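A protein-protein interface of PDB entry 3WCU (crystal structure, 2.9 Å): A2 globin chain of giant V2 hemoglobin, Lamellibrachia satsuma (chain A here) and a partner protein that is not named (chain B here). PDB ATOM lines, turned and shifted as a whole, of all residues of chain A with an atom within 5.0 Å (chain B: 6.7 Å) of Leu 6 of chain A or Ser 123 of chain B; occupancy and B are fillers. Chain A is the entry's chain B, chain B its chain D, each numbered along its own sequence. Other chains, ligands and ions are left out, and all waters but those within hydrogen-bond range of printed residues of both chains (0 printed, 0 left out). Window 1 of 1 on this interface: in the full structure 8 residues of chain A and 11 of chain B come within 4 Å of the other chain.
O of Pro 122 of chain B sits at hydrogen-bond distance from NZ of Lys 10 of chain A, 3.0 Å away.
O of Ile 125 of chain B sits at hydrogen-bond distance from NZ of Lys 10 of chain A.
NZ of Lys 10 of chain A lies within salt-bridge range of OD1 of Asp 126 of chain A, at 3.9 Å.
Among the printed residues, pairs that only touch across the chains: Pro 5 of chain A with Thr 31 of chain B (3.4 Å), Pro 5 of chain A with Glu 35 of chain B (3.2 Å), Leu 6 of chain A with Glu 35 of chain B (3.6 Å), Leu 6 of chain A with Val 120 of chain B (3.9 Å), Leu 6 of chain A with Ser 123 of chain B (3.7 Å), Leu 6 of chain A with Leu 124 of chain B (3.7 Å), Leu 9 of chain A with Leu 124 of chain B (3.9 Å), Lys 10 of chain A with Ser 123 of chain B (3.0 Å) and Lys 10 of chain A with Leu 124 of chain B (3.5 Å).
Ser 123 of chain B touches just these residues of chain A: Leu 6 (3.7 Å) and Lys 10 (3.0 Å).
Printed residues of chain B within 4 Å of Lys 10 of chain A: Pro 122, Ser 123, Leu 124 and Ile 125.
Of the printed residues of chain A, Pro 122 of chain B touches Lys 10.
Asp 126 of chain B touches none of the printed residues of chain A.
Asp 126 of chain A touches none of the printed residues of chain B.
The nearest residue of chain B that does not touch Leu 6 of chain A is Thr 31 of chain B (4.6 Å).
Among the printed residues, 11 pairs touch across the chains.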
ATOM      1  N   GLY A   4       1.605  19.987 -25.451  1.00  0.00           N
ATOM      2  CA  GLY A   4       1.421  20.752 -26.676  1.00  0.00           C
ATOM      3  C   GLY A   4       1.752  22.237 -26.582  1.00  0.00           C
ATOM      4  O   GLY A   4       2.397  22.668 -25.626  1.00  0.00           O
ATOM      5  N   PRO A   5       1.327  23.051 -27.569  1.00  0.00           N
ATOM      6  CA  PRO A   5       1.587  24.496 -27.593  1.00  0.00           C
ATOM      7  C   PRO A   5       0.721  25.222 -26.586  1.00  0.00           C
ATOM      8  O   PRO A   5       1.202  26.079 -25.851  1.00  0.00           O
ATOM      9  CB  PRO A   5       1.221  24.904 -29.024  1.00  0.00           C
ATOM     10  CG  PRO A   5       1.214  23.618 -29.792  1.00  0.00           C
ATOM     11  CD  PRO A   5       0.650  22.638 -28.807  1.00  0.00           C
ATOM     12  N   LEU A   6      -0.565  24.869 -26.582  1.00  0.00           N
ATOM     13  CA  LEU A   6      -1.543  25.470 -25.683  1.00  0.00           C
ATOM     14  C   LEU A   6      -1.125  25.235 -24.234  1.00  0.00           C
ATOM     15  O   LEU A   6      -1.029  26.182 -23.451  1.00  0.00           O
ATOM     16  CB  LEU A   6      -2.949  24.883 -25.945  1.00  0.00           C
ATOM     17  CG  LEU A   6      -3.662  25.189 -27.290  1.00  0.00           C
ATOM     18  CD1 LEU A   6      -4.968  24.413 -27.380  1.00  0.00           C
ATOM     19  CD2 LEU A   6      -3.936  26.682 -27.437  1.00  0.00           C
ATOM     20  N   GLN A   7      -0.852  23.975 -23.894  1.00  0.00           N
ATOM     21  CA  GLN A   7      -0.448  23.588 -22.539  1.00  0.00           C
ATOM     22  C   GLN A   7       0.797  24.316 -22.032  1.00  0.00           C
ATOM     23  O   GLN A   7       0.990  24.456 -20.827  1.00  0.00           O
ATOM     24  CB  GLN A   7      -0.182  22.076 -22.456  1.00  0.00           C
ATOM     25  CG  GLN A   7      -1.353  21.164 -22.782  1.00  0.00           C
ATOM     26  CD  GLN A   7      -1.722  21.155 -24.263  1.00  0.00           C
ATOM     27  OE1 GLN A   7      -0.894  21.439 -25.137  1.00  0.00           O
ATOM     28  NE2 GLN A   7      -2.972  20.802 -24.551  1.00  0.00           N
ATOM     29  N   ARG A   8       1.661  24.755 -22.939  1.00  0.00           N
ATOM     30  CA  ARG A   8       2.878  25.445 -22.522  1.00  0.00           C
ATOM     31  C   ARG A   8       2.584  26.884 -22.132  1.00  0.00           C
ATOM     32  O   ARG A   8       3.262  27.462 -21.286  1.00  0.00           O
ATOM     33  CB  ARG A   8       3.928  25.399 -23.641  1.00  0.00           C
ATOM     34  CG  ARG A   8       4.604  24.048 -23.798  1.00  0.00           C
ATOM     35  CD  ARG A   8       5.088  23.838 -25.222  1.00  0.00           C
ATOM     36  NE  ARG A   8       5.522  22.461 -25.430  1.00  0.00           N
ATOM     37  CZ  ARG A   8       6.753  22.009 -25.203  1.00  0.00           C
ATOM     38  NH1 ARG A   8       7.704  22.823 -24.766  1.00  0.00           N
ATOM     39  NH2 ARG A   8       7.027  20.727 -25.394  1.00  0.00           N
ATOM     40  N   LEU A   9       1.563  27.463 -22.754  1.00  0.00           N
ATOM     41  CA  LEU A   9       1.184  28.826 -22.449  1.00  0.00           C
ATOM     42  C   LEU A   9       0.515  28.843 -21.107  1.00  0.00           C
ATOM     43  O   LEU A   9       0.904  29.615 -20.250  1.00  0.00           O
ATOM     44  CB  LEU A   9       0.241  29.369 -23.504  1.00  0.00           C
ATOM     45  CG  LEU A   9       0.951  29.667 -24.817  1.00  0.00           C
ATOM     46  CD1 LEU A   9      -0.006  30.408 -25.754  1.00  0.00           C
ATOM     47  CD2 LEU A   9       2.205  30.496 -24.538  1.00  0.00           C
ATOM     48  N   LYS A  10      -0.478  27.977 -20.914  1.00  0.00           N
ATOM     49  CA  LYS A  10      -1.184  27.926 -19.639  1.00  0.00           C
ATOM     50  C   LYS A  10      -0.272  27.571 -18.486  1.00  0.00           C
ATOM     51  O   LYS A  10      -0.592  27.862 -17.336  1.00  0.00           O
ATOM     52  CB  LYS A  10      -2.340  26.924 -19.663  1.00  0.00           C
ATOM     53  CG  LYS A  10      -2.876  26.627 -18.264  1.00  0.00           C
ATOM     54  CD  LYS A  10      -4.103  25.736 -18.275  1.00  0.00           C
ATOM     55  CE  LYS A  10      -5.341  26.489 -18.717  1.00  0.00           C
ATOM     56  NZ  LYS A  10      -6.558  25.674 -18.497  1.00  0.00           N
ATOM     57  N   ASP A 126      -4.175  22.927 -13.640  1.00  0.00           N
ATOM     58  CA  ASP A 126      -4.346  21.986 -14.766  1.00  0.00           C
ATOM     59  C   ASP A 126      -3.264  20.896 -14.730  1.00  0.00           C
ATOM     60  O   ASP A 126      -2.161  21.081 -15.248  1.00  0.00           O
ATOM     61  CB  ASP A 126      -4.284  22.753 -16.097  1.00  0.00           C
ATOM     62  CG  ASP A 126      -4.450  21.852 -17.303  1.00  0.00           C
ATOM     63  OD1 ASP A 126      -4.489  22.376 -18.442  1.00  0.00           O
ATOM     64  OD2 ASP A 126      -4.539  20.623 -17.105  1.00  0.00           O
ATOM     65  N   THR B  31       0.758  31.282 -31.764  1.00  0.00           N
ATOM     66  CA  THR B  31       0.354  29.961 -31.315  1.00  0.00           C
ATOM     67  C   THR B  31      -1.168  29.835 -31.254  1.00  0.00           C
ATOM     68  O   THR B  31      -1.723  28.772 -31.546  1.00  0.00           O
ATOM     69  CB  THR B  31       0.977  29.637 -29.941  1.00  0.00           C
ATOM     70  OG1 THR B  31       2.396  29.830 -30.010  1.00  0.00           O
ATOM     71  CG2 THR B  31       0.692  28.194 -29.544  1.00  0.00           C
ATOM     72  N   MET B  32      -1.851  30.919 -30.894  1.00  0.00           N
ATOM     73  CA  MET B  32      -3.311  30.894 -30.823  1.00  0.00           C
ATOM     74  C   MET B  32      -3.936  30.917 -32.214  1.00  0.00           C
ATOM     75  O   MET B  32      -4.862  30.154 -32.503  1.00  0.00           O
ATOM     76  CB  MET B  32      -3.823  32.074 -30.000  1.00  0.00           C
ATOM     77  CG  MET B  32      -3.629  31.892 -28.510  1.00  0.00           C
ATOM     78  SD  MET B  32      -4.173  33.323 -27.600  1.00  0.00           S
ATOM     79  CE  MET B  32      -5.935  33.300 -27.939  1.00  0.00           C
ATOM     80  N   GLU B  35      -3.355  27.372 -33.744  1.00  0.00           N
ATOM     81  CA  GLU B  35      -4.226  26.474 -32.990  1.00  0.00           C
ATOM     82  C   GLU B  35      -5.697  26.571 -33.395  1.00  0.00           C
ATOM     83  O   GLU B  35      -6.334  25.555 -33.684  1.00  0.00           O
ATOM     84  CB  GLU B  35      -4.105  26.775 -31.503  1.00  0.00           C
ATOM     85  CG  GLU B  35      -2.871  26.209 -30.877  1.00  0.00           C
ATOM     86  CD  GLU B  35      -2.788  24.731 -31.102  1.00  0.00           C
ATOM     87  OE1 GLU B  35      -3.862  24.097 -31.196  1.00  0.00           O
ATOM     88  OE2 GLU B  35      -1.659  24.207 -31.174  1.00  0.00           O
ATOM     89  N   ILE B  36      -6.220  27.799 -33.412  1.00  0.00           N
ATOM     90  CA  ILE B  36      -7.615  28.055 -33.758  1.00  0.00           C
ATOM     91  C   ILE B  36      -7.979  27.694 -35.191  1.00  0.00           C
ATOM     92  O   ILE B  36      -9.085  27.231 -35.445  1.00  0.00           O
ATOM     93  CB  ILE B  36      -8.001  29.544 -33.516  1.00  0.00           C
ATOM     94  CG1 ILE B  36      -8.057  29.842 -32.015  1.00  0.00           C
ATOM     95  CG2 ILE B  36      -9.366  29.838 -34.120  1.00  0.00           C
ATOM     96  CD1 ILE B  36      -8.184  31.319 -31.706  1.00  0.00           C
ATOM     97  N   SER B  39      -7.466  23.932 -36.178  1.00  0.00           N
ATOM     98  CA  SER B  39      -8.545  23.179 -35.552  1.00  0.00           C
ATOM     99  C   SER B  39      -9.823  23.420 -36.340  1.00  0.00           C
ATOM    100  O   SER B  39     -10.713  22.568 -36.386  1.00  0.00           O
ATOM    101  CB  SER B  39      -8.735  23.629 -34.102  1.00  0.00           C
ATOM    102  OG  SER B  39      -7.508  23.607 -33.393  1.00  0.00           O
ATOM    103  N   MET B 118     -14.599  27.058 -28.303  1.00  0.00           N
ATOM    104  CA  MET B 118     -15.085  26.387 -27.098  1.00  0.00           C
ATOM    105  C   MET B 118     -14.150  25.287 -26.616  1.00  0.00           C
ATOM    106  O   MET B 118     -14.059  25.024 -25.414  1.00  0.00           O
ATOM    107  CB  MET B 118     -16.457  25.768 -27.340  1.00  0.00           C
ATOM    108  CG  MET B 118     -17.573  26.760 -27.375  1.00  0.00           C
ATOM    109  SD  MET B 118     -17.728  27.620 -25.814  1.00  0.00           S
ATOM    110  CE  MET B 118     -18.055  29.281 -26.439  1.00  0.00           C
ATOM    111  N   THR B 119     -13.454  24.652 -27.557  1.00  0.00           N
ATOM    112  CA  THR B 119     -12.555  23.551 -27.234  1.00  0.00           C
ATOM    113  C   THR B 119     -11.133  24.055 -27.003  1.00  0.00           C
ATOM    114  O   THR B 119     -10.419  23.590 -26.113  1.00  0.00           O
ATOM    115  CB  THR B 119     -12.530  22.516 -28.377  1.00  0.00           C
ATOM    116  OG1 THR B 119     -13.860  22.280 -28.846  1.00  0.00           O
ATOM    117  CG2 THR B 119     -11.991  21.193 -27.882  1.00  0.00           C
ATOM    118  N   VAL B 120     -10.726  25.021 -27.804  1.00  0.00           N
ATOM    119  CA  VAL B 120      -9.384  25.554 -27.676  1.00  0.00           C
ATOM    120  C   VAL B 120      -9.138  26.386 -26.423  1.00  0.00           C
ATOM    121  O   VAL B 120      -8.211  26.110 -25.656  1.00  0.00           O
ATOM    122  CB  VAL B 120      -9.006  26.409 -28.909  1.00  0.00           C
ATOM    123  CG1 VAL B 120      -7.650  27.054 -28.708  1.00  0.00           C
ATOM    124  CG2 VAL B 120      -9.009  25.544 -30.138  1.00  0.00           C
ATOM    125  N   LEU B 121      -9.987  27.378 -26.189  1.00  0.00           N
ATOM    126  CA  LEU B 121      -9.761  28.280 -25.074  1.00  0.00           C
ATOM    127  C   LEU B 121      -9.560  27.687 -23.706  1.00  0.00           C
ATOM    128  O   LEU B 121      -8.655  28.095 -22.982  1.00  0.00           O
ATOM    129  CB  LEU B 121     -10.866  29.334 -25.011  1.00  0.00           C
ATOM    130  CG  LEU B 121     -11.006  30.324 -26.179  1.00  0.00           C
ATOM    131  CD1 LEU B 121     -12.251  31.194 -25.996  1.00  0.00           C
ATOM    132  CD2 LEU B 121      -9.772  31.191 -26.260  1.00  0.00           C
ATOM    133  N   PRO B 122     -10.387  26.714 -23.335  1.00  0.00           N
ATOM    134  CA  PRO B 122     -10.226  26.119 -22.009  1.00  0.00           C
ATOM    135  C   PRO B 122      -8.860  25.546 -21.750  1.00  0.00           C
ATOM    136  O   PRO B 122      -8.557  25.179 -20.627  1.00  0.00           O
ATOM    137  CB  PRO B 122     -11.342  25.084 -21.932  1.00  0.00           C
ATOM    138  CG  PRO B 122     -11.821  24.931 -23.335  1.00  0.00           C
ATOM    139  CD  PRO B 122     -11.618  26.258 -23.992  1.00  0.00           C
ATOM    140  N   SER B 123      -8.024  25.482 -22.777  1.00  0.00           N
ATOM    141  CA  SER B 123      -6.673  24.979 -22.589  1.00  0.00           C
ATOM    142  C   SER B 123      -5.769  26.143 -22.181  1.00  0.00           C
ATOM    143  O   SER B 123      -4.692  25.942 -21.617  1.00  0.00           O
ATOM    144  CB  SER B 123      -6.162  24.325 -23.875  1.00  0.00           C
ATOM    145  OG  SER B 123      -6.888  23.140 -24.165  1.00  0.00           O
ATOM    146  N   LEU B 124      -6.229  27.363 -22.449  1.00  0.00           N
ATOM    147  CA  LEU B 124      -5.469  28.568 -22.118  1.00  0.00           C
ATOM    148  C   LEU B 124      -5.961  29.292 -20.857  1.00  0.00           C
ATOM    149  O   LEU B 124      -5.149  29.769 -20.059  1.00  0.00           O
ATOM    150  CB  LEU B 124      -5.502  29.534 -23.302  1.00  0.00           C
ATOM    151  CG  LEU B 124      -4.956  29.035 -24.643  1.00  0.00           C
ATOM    152  CD1 LEU B 124      -5.386  29.974 -25.749  1.00  0.00           C
ATOM    153  CD2 LEU B 124      -3.449  28.942 -24.596  1.00  0.00           C
ATOM    154  N   ILE B 125      -7.285  29.354 -20.688  1.00  0.00           N
ATOM    155  CA  ILE B 125      -7.945  30.025 -19.551  1.00  0.00           C
ATOM    156  C   ILE B 125      -8.147  29.178 -18.278  1.00  0.00           C
ATOM    157  O   ILE B 125      -8.506  28.002 -18.355  1.00  0.00           O
ATOM    158  CB  ILE B 125      -9.343  30.565 -19.976  1.00  0.00           C
ATOM    159  CG1 ILE B 125      -9.188  31.691 -20.993  1.00  0.00           C
ATOM    160  CG2 ILE B 125     -10.113  31.062 -18.774  1.00  0.00           C
ATOM    161  CD1 ILE B 125     -10.517  32.278 -21.458  1.00  0.00           C
ATOM    162  N   ASP B 126      -7.932  29.790 -17.111  1.00  0.00           N
ATOM    163  CA  ASP B 126      -8.108  29.104 -15.830  1.00  0.00           C
ATOM    164  C   ASP B 126      -9.595  28.991 -15.513  1.00  0.00           C
ATOM    165  O   ASP B 126     -10.337  29.980 -15.598  1.00  0.00           O
ATOM    166  CB  ASP B 126      -7.442  29.874 -14.679  1.00  0.00           C
ATOM    167  CG  ASP B 126      -5.976  30.142 -14.917  1.00  0.00           C
ATOM    168  OD1 ASP B 126      -5.494  29.841 -16.023  1.00  0.00           O
ATOM    169  OD2 ASP B 126      -5.301  30.664 -14.003  1.00  0.00           O
ATOM    170  N   PHE B 128     -12.027  27.991 -17.085  1.00  0.00           N
ATOM    171  CA  PHE B 128     -12.856  28.487 -18.185  1.00  0.00           C
ATOM    172  C   PHE B 128     -14.314  28.130 -17.914  1.00  0.00           C
ATOM    173  O   PHE B 128     -14.609  27.018 -17.486  1.00  0.00           O
ATOM    174  CB  PHE B 128     -12.384  27.842 -19.489  1.00  0.00           C
ATOM    175  CG  PHE B 128     -13.260  28.126 -20.676  1.00  0.00           C
ATOM    176  CD1 PHE B 128     -13.105  29.295 -21.412  1.00  0.00           C
ATOM    177  CD2 PHE B 128     -14.219  27.209 -21.077  1.00  0.00           C
ATOM    178  CE1 PHE B 128     -13.903  29.538 -22.542  1.00  0.00           C
ATOM    179  CE2 PHE B 128     -15.009  27.446 -22.192  1.00  0.00           C
ATOM    180  CZ  PHE B 128     -14.854  28.606 -22.926  1.00  0.00           C
